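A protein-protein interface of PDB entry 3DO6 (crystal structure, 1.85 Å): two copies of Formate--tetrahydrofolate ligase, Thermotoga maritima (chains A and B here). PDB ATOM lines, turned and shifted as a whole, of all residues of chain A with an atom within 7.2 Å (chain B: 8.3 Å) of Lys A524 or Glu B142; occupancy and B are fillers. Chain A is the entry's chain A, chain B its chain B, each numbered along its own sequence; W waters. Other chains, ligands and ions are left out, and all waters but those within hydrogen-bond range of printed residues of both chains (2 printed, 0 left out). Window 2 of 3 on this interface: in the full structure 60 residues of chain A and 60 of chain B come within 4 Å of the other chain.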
ATOM      1  N   ARG A 161      10.750  30.225 -17.630  1.00  0.00           N
ATOM      2  CA  ARG A 161      11.795  30.965 -18.315  1.00  0.00           C
ATOM      3  C   ARG A 161      11.456  31.264 -19.775  1.00  0.00           C
ATOM      4  O   ARG A 161      11.975  32.209 -20.327  1.00  0.00           O
ATOM      5  CB  ARG A 161      13.138  30.217 -18.240  1.00  0.00           C
ATOM      6  CG  ARG A 161      13.144  28.894 -18.986  1.00  0.00           C
ATOM      7  CD  ARG A 161      14.508  28.222 -19.062  1.00  0.00           C
ATOM      8  NE  ARG A 161      15.020  27.842 -17.774  1.00  0.00           N
ATOM      9  CZ  ARG A 161      14.689  26.714 -17.154  1.00  0.00           C
ATOM     10  NH1 ARG A 161      13.827  25.879 -17.729  1.00  0.00           N
ATOM     11  NH2 ARG A 161      15.225  26.430 -15.967  1.00  0.00           N
ATOM     12  N   LEU A 522      12.500  26.423 -14.006  1.00  0.00           N
ATOM     13  CA  LEU A 522      12.326  25.092 -13.393  1.00  0.00           C
ATOM     14  C   LEU A 522      13.594  24.256 -13.527  1.00  0.00           C
ATOM     15  O   LEU A 522      14.267  24.280 -14.559  1.00  0.00           O
ATOM     16  CB  LEU A 522      11.149  24.340 -14.036  1.00  0.00           C
ATOM     17  CG  LEU A 522       9.743  24.838 -13.672  1.00  0.00           C
ATOM     18  CD1 LEU A 522       8.707  24.178 -14.603  1.00  0.00           C
ATOM     19  CD2 LEU A 522       9.441  24.558 -12.212  1.00  0.00           C
ATOM     20  N   PRO A 523      13.932  23.487 -12.485  1.00  0.00           N
ATOM     21  CA  PRO A 523      15.057  22.540 -12.591  1.00  0.00           C
ATOM     22  C   PRO A 523      14.731  21.341 -13.473  1.00  0.00           C
ATOM     23  O   PRO A 523      13.583  21.134 -13.841  1.00  0.00           O
ATOM     24  CB  PRO A 523      15.308  22.128 -11.134  1.00  0.00           C
ATOM     25  CG  PRO A 523      14.081  22.458 -10.406  1.00  0.00           C
ATOM     26  CD  PRO A 523      13.256  23.406 -11.186  1.00  0.00           C
ATOM     27  N   LYS A 524      15.762  20.592 -13.825  1.00  0.00           N
ATOM     28  CA  LYS A 524      15.623  19.431 -14.699  1.00  0.00           C
ATOM     29  C   LYS A 524      14.602  18.430 -14.129  1.00  0.00           C
ATOM     30  O   LYS A 524      13.800  17.876 -14.864  1.00  0.00           O
ATOM     31  CB  LYS A 524      16.960  18.763 -15.000  1.00  0.00           C
ATOM     32  CG  LYS A 524      16.757  17.661 -16.001  1.00  0.00           C
ATOM     33  CD  LYS A 524      18.022  17.072 -16.567  1.00  0.00           C
ATOM     34  CE  LYS A 524      17.630  16.087 -17.665  1.00  0.00           C
ATOM     35  NZ  LYS A 524      18.437  16.246 -18.878  1.00  0.00           N
ATOM     36  N   LYS A 525      14.595  18.286 -12.809  1.00  0.00           N
ATOM     37  CA  LYS A 525      13.635  17.406 -12.119  1.00  0.00           C
ATOM     38  C   LYS A 525      12.825  18.227 -11.146  1.00  0.00           C
ATOM     39  O   LYS A 525      13.184  18.370  -9.981  1.00  0.00           O
ATOM     40  CB  LYS A 525      14.330  16.279 -11.341  1.00  0.00           C
ATOM     41  CG  LYS A 525      15.181  15.390 -12.192  1.00  0.00           C
ATOM     42  CD  LYS A 525      14.385  14.470 -13.087  1.00  0.00           C
ATOM     43  CE  LYS A 525      15.321  13.763 -14.085  1.00  0.00           C
ATOM     44  NZ  LYS A 525      14.570  13.070 -15.163  1.00  0.00           N
ATOM     45  N   PRO A 526      11.738  18.800 -11.624  1.00  0.00           N
ATOM     46  CA  PRO A 526      11.009  19.683 -10.734  1.00  0.00           C
ATOM     47  C   PRO A 526      10.250  18.938  -9.650  1.00  0.00           C
ATOM     48  O   PRO A 526       9.862  17.765  -9.818  1.00  0.00           O
ATOM     49  CB  PRO A 526      10.042  20.403 -11.651  1.00  0.00           C
ATOM     50  CG  PRO A 526      10.067  19.735 -12.933  1.00  0.00           C
ATOM     51  CD  PRO A 526      11.187  18.757 -12.973  1.00  0.00           C
ATOM     52  N   LEU A 529       7.088  16.856  -9.845  1.00  0.00           N
ATOM     53  CA  LEU A 529       7.135  15.409 -10.164  1.00  0.00           C
ATOM     54  C   LEU A 529       6.717  14.589  -8.922  1.00  0.00           C
ATOM     55  O   LEU A 529       6.207  13.482  -9.032  1.00  0.00           O
ATOM     56  CB  LEU A 529       8.522  14.983 -10.690  1.00  0.00           C
ATOM     57  CG  LEU A 529       8.917  15.464 -12.092  1.00  0.00           C
ATOM     58  CD1 LEU A 529      10.398  15.195 -12.429  1.00  0.00           C
ATOM     59  CD2 LEU A 529       8.051  14.858 -13.151  1.00  0.00           C
ATOM     60  N   VAL B 132       6.495  23.155 -17.855  1.00  0.00           N
ATOM     61  CA  VAL B 132       7.236  21.888 -17.748  1.00  0.00           C
ATOM     62  C   VAL B 132       7.667  21.350 -19.112  1.00  0.00           C
ATOM     63  O   VAL B 132       8.751  20.801 -19.251  1.00  0.00           O
ATOM     64  CB  VAL B 132       6.433  20.804 -16.946  1.00  0.00           C
ATOM     65  CG1 VAL B 132       7.046  19.409 -17.128  1.00  0.00           C
ATOM     66  CG2 VAL B 132       6.372  21.204 -15.480  1.00  0.00           C
ATOM     67  N   SER B 135      10.562  23.472 -20.315  1.00  0.00           N
ATOM     68  CA  SER B 135      11.735  23.213 -19.482  1.00  0.00           C
ATOM     69  C   SER B 135      12.351  21.831 -19.798  1.00  0.00           C
ATOM     70  O   SER B 135      13.582  21.674 -19.817  1.00  0.00           O
ATOM     71  CB  SER B 135      11.368  23.351 -17.993  1.00  0.00           C
ATOM     72  OG  SER B 135      12.479  23.215 -17.146  1.00  0.00           O
ATOM     73  N   HIS B 136      11.490  20.874 -20.101  1.00  0.00           N
ATOM     74  CA  HIS B 136      11.912  19.527 -20.547  1.00  0.00           C
ATOM     75  C   HIS B 136      12.765  19.693 -21.804  1.00  0.00           C
ATOM     76  O   HIS B 136      13.857  19.116 -21.946  1.00  0.00           O
ATOM     77  CB  HIS B 136      10.718  18.580 -20.824  1.00  0.00           C
ATOM     78  CG  HIS B 136      11.134  17.249 -21.391  1.00  0.00           C
ATOM     79  ND1 HIS B 136      11.564  16.203 -20.598  1.00  0.00           N
ATOM     80  CD2 HIS B 136      11.243  16.817 -22.671  1.00  0.00           C
ATOM     81  CE1 HIS B 136      11.909  15.182 -21.369  1.00  0.00           C
ATOM     82  NE2 HIS B 136      11.710  15.524 -22.630  1.00  0.00           N
ATOM     83  N   ILE B 137      12.262  20.518 -22.705  1.00  0.00           N
ATOM     84  CA  ILE B 137      12.965  20.738 -23.985  1.00  0.00           C
ATOM     85  C   ILE B 137      14.316  21.406 -23.709  1.00  0.00           C
ATOM     86  O   ILE B 137      15.355  21.010 -24.232  1.00  0.00           O
ATOM     87  CB  ILE B 137      12.119  21.534 -24.977  1.00  0.00           C
ATOM     88  CG1 ILE B 137      10.887  20.701 -25.372  1.00  0.00           C
ATOM     89  CG2 ILE B 137      12.980  21.913 -26.222  1.00  0.00           C
ATOM     90  CD1 ILE B 137       9.802  21.494 -26.133  1.00  0.00           C
ATOM     91  N   LYS B 138      14.298  22.378 -22.814  1.00  0.00           N
ATOM     92  CA  LYS B 138      15.494  23.148 -22.513  1.00  0.00           C
ATOM     93  C   LYS B 138      16.601  22.275 -21.957  1.00  0.00           C
ATOM     94  O   LYS B 138      17.783  22.482 -22.245  1.00  0.00           O
ATOM     95  CB  LYS B 138      15.208  24.255 -21.532  1.00  0.00           C
ATOM     96  CG  LYS B 138      16.421  25.162 -21.261  1.00  0.00           C
ATOM     97  CD  LYS B 138      16.868  25.028 -19.820  1.00  0.00           C
ATOM     98  CE  LYS B 138      18.016  25.990 -19.507  1.00  0.00           C
ATOM     99  NZ  LYS B 138      19.243  25.452 -20.127  1.00  0.00           N
ATOM    100  N   HIS B 139      16.193  21.345 -21.120  1.00  0.00           N
ATOM    101  CA  HIS B 139      17.120  20.510 -20.356  1.00  0.00           C
ATOM    102  C   HIS B 139      17.496  19.220 -21.040  1.00  0.00           C
ATOM    103  O   HIS B 139      17.899  18.293 -20.386  1.00  0.00           O
ATOM    104  CB  HIS B 139      16.544  20.119 -18.989  1.00  0.00           C
ATOM    105  CG  HIS B 139      16.484  21.230 -18.013  1.00  0.00           C
ATOM    106  ND1 HIS B 139      17.599  21.779 -17.423  1.00  0.00           N
ATOM    107  CD2 HIS B 139      15.423  21.868 -17.477  1.00  0.00           C
ATOM    108  CE1 HIS B 139      17.226  22.728 -16.588  1.00  0.00           C
ATOM    109  NE2 HIS B 139      15.910  22.798 -16.602  1.00  0.00           N
ATOM    110  N   GLY B 140      17.342  19.142 -22.346  1.00  0.00           N
ATOM    111  CA  GLY B 140      17.857  17.994 -23.112  1.00  0.00           C
ATOM    112  C   GLY B 140      16.872  17.357 -24.061  1.00  0.00           C
ATOM    113  O   GLY B 140      17.239  16.554 -24.929  1.00  0.00           O
ATOM    114  N   ASN B 141      15.609  17.707 -23.886  1.00  0.00           N
ATOM    115  CA  ASN B 141      14.524  17.212 -24.718  1.00  0.00           C
ATOM    116  C   ASN B 141      14.626  15.689 -24.961  1.00  0.00           C
ATOM    117  O   ASN B 141      14.634  15.206 -26.093  1.00  0.00           O
ATOM    118  CB  ASN B 141      14.522  17.963 -26.035  1.00  0.00           C
ATOM    119  CG  ASN B 141      13.244  17.792 -26.800  1.00  0.00           C
ATOM    120  OD1 ASN B 141      12.274  17.298 -26.269  1.00  0.00           O
ATOM    121  ND2 ASN B 141      13.236  18.207 -28.071  1.00  0.00           N
ATOM    122  N   GLU B 142      14.704  14.945 -23.867  1.00  0.00           N
ATOM    123  CA  GLU B 142      14.820  13.502 -23.964  1.00  0.00           C
ATOM    124  C   GLU B 142      13.616  12.871 -24.647  1.00  0.00           C
ATOM    125  O   GLU B 142      13.739  11.845 -25.259  1.00  0.00           O
ATOM    126  CB  GLU B 142      15.058  12.856 -22.609  1.00  0.00           C
ATOM    127  CG  GLU B 142      16.483  13.058 -22.126  1.00  0.00           C
ATOM    128  CD  GLU B 142      16.589  14.187 -21.147  1.00  0.00           C
ATOM    129  OE1 GLU B 142      15.660  15.051 -21.163  1.00  0.00           O
ATOM    130  OE2 GLU B 142      17.579  14.203 -20.371  1.00  0.00           O
ATOM    131  N   LEU B 143      12.468  13.528 -24.566  1.00  0.00           N
ATOM    132  CA  LEU B 143      11.242  13.037 -25.201  1.00  0.00           C
ATOM    133  C   LEU B 143      11.202  13.334 -26.713  1.00  0.00           C
ATOM    134  O   LEU B 143      10.265  12.983 -27.403  1.00  0.00           O
ATOM    135  CB  LEU B 143       9.978  13.597 -24.517  1.00  0.00           C
ATOM    136  CG  LEU B 143       9.575  12.992 -23.151  1.00  0.00           C
ATOM    137  CD1 LEU B 143       8.428  13.800 -22.442  1.00  0.00           C
ATOM    138  CD2 LEU B 143       9.171  11.523 -23.297  1.00  0.00           C
ATOM    139  N   LYS B 144      12.205  14.054 -27.176  1.00  0.00           N
ATOM    140  CA  LYS B 144      12.343  14.451 -28.587  1.00  0.00           C
ATOM    141  C   LYS B 144      11.115  15.144 -29.121  1.00  0.00           C
ATOM    142  O   LYS B 144      10.667  14.887 -30.243  1.00  0.00           O
ATOM    143  CB  LYS B 144      12.677  13.225 -29.450  1.00  0.00           C
ATOM    144  CG  LYS B 144      13.930  12.505 -28.985  1.00  0.00           C
ATOM    145  CD  LYS B 144      14.230  11.270 -29.850  1.00  0.00           C
ATOM    146  N   ILE B 145      10.564  16.025 -28.291  1.00  0.00           N
ATOM    147  CA  ILE B 145       9.396  16.834 -28.676  1.00  0.00           C
ATOM    148  C   ILE B 145       9.729  17.708 -29.882  1.00  0.00           C
ATOM    149  O   ILE B 145      10.748  18.386 -29.902  1.00  0.00           O
ATOM    150  CB  ILE B 145       8.870  17.710 -27.496  1.00  0.00           C
ATOM    151  CG1 ILE B 145       8.311  16.792 -26.378  1.00  0.00           C
ATOM    152  CG2 ILE B 145       7.770  18.710 -27.993  1.00  0.00           C
ATOM    153  CD1 ILE B 145       8.072  17.496 -25.084  1.00  0.00           C
ATOM    154  N   ASP B 216       6.387  13.843 -31.190  1.00  0.00           N
ATOM    155  CA  ASP B 216       7.835  13.787 -31.157  1.00  0.00           C
ATOM    156  C   ASP B 216       8.435  13.713 -32.554  1.00  0.00           C
ATOM    157  O   ASP B 216       7.732  13.793 -33.576  1.00  0.00           O
ATOM    158  CB  ASP B 216       8.388  12.670 -30.246  1.00  0.00           C
ATOM    159  CG  ASP B 216       8.199  11.246 -30.816  1.00  0.00           C
ATOM    160  OD1 ASP B 216       7.785  11.057 -31.976  1.00  0.00           O
ATOM    161  OD2 ASP B 216       8.460  10.304 -30.054  1.00  0.00           O
ATOM    162  N   VAL B 222       2.984  12.410 -27.708  1.00  0.00           N
ATOM    163  CA  VAL B 222       3.472  12.696 -26.363  1.00  0.00           C
ATOM    164  C   VAL B 222       2.268  13.166 -25.510  1.00  0.00           C
ATOM    165  O   VAL B 222       1.537  14.096 -25.866  1.00  0.00           O
ATOM    166  CB  VAL B 222       4.615  13.744 -26.334  1.00  0.00           C
ATOM    167  CG1 VAL B 222       5.078  13.987 -24.892  1.00  0.00           C
ATOM    168  CG2 VAL B 222       5.791  13.341 -27.255  1.00  0.00           C
ATOM    169  N   LEU B 227       5.265  13.169 -19.278  1.00  0.00           N
ATOM    170  CA  LEU B 227       5.987  14.212 -18.560  1.00  0.00           C
ATOM    171  C   LEU B 227       5.848  14.022 -17.064  1.00  0.00           C
ATOM    172  O   LEU B 227       6.637  14.549 -16.289  1.00  0.00           O
ATOM    173  CB  LEU B 227       5.471  15.609 -18.935  1.00  0.00           C
ATOM    174  CG  LEU B 227       5.923  16.111 -20.315  1.00  0.00           C
ATOM    175  CD1 LEU B 227       5.001  17.220 -20.830  1.00  0.00           C
ATOM    176  CD2 LEU B 227       7.400  16.540 -20.250  1.00  0.00           C
HETATM  177  O   HOH W   1      12.364  20.862 -16.164  1.00  0.00           O
HETATM  178  O   HOH W   2      12.045  26.267 -20.056  1.00  0.00           O
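The guanidinium group (NH1) of Arg A161 lies within hydrogen-bond range of the side-chain hydroxyl (OG) of Ser B135, 3.0 Å away.
OG of Ser B135 is in hydrogen-bond range of O of Leu A522 (3.3 Å).
O of Leu A522 is in hydrogen-bond range of NE2 of His B139 (3.0 Å).
NZ of Lys A524 sits at hydrogen-bond distance from O of His B139, at 2.6 Å.
NZ of Lys A524 is in salt-bridge range of OE2 of Glu B142, 2.7 Å away.
NH2 of Arg A161 sits at hydrogen-bond distance from O of Leu A522, at 2.7 Å.
NE2 of His B139 sits close to OG of Ser B135, at 3.5 Å.
The backbone NH (N) of Glu B142 is in hydrogen-bond range of a ring nitrogen (NE2) of His B136 (3.3 Å).
Among the printed residues, pairs that only touch across the chains: Arg A161 with Lys B138 (3.8 Å), Arg A161 with His B139 (3.8 Å), Leu A522 with Val B132 (3.9 Å), Pro A523 with His B139 (3.6 Å) and Leu A529 with Leu B227 (3.5 Å).
Of the printed residues of chain B, Arg A161 touches Ser B135, Lys B138 and His B139.
Lys A524 touches just these residues of chain B: His B139 and Glu B142.
Printed residues of chain B within 4 Å of Leu A529: Leu B227 (3.5 Å).
Of chain A, only Lys A524 comes within 4 Å of Glu B142.
The nearest residue of chain A that does not touch Glu B142 is Lys A525 (6.1 Å).
The nearest printed residue of chain A that does not touch Ser B135 is Pro A523 (4.1 Å).
Of the 15 printed residues of chain B, 6 touch a printed residue of chain A.
Hydrophobic or aromatic side chains of chain B that line the printed part of chain A: Val B132 and His B139.
Of the 7 printed residues of chain A, 5 touch a printed residue of chain B.
Hydrophobic or aromatic side chains of chain A that line the printed part of chain B: Leu A522 and Leu A529.
No position is printed for both chains.
Water W1 bridges the side-chain hydroxyl of Ser B135 (2.6 Å) and the backbone carbonyl oxygen of Pro A523 (2.6 Å).
Water W2 bridges the guanidinium group of Arg A161 (3.0 Å) and the backbone NH of Ser B135 (3.2 Å).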
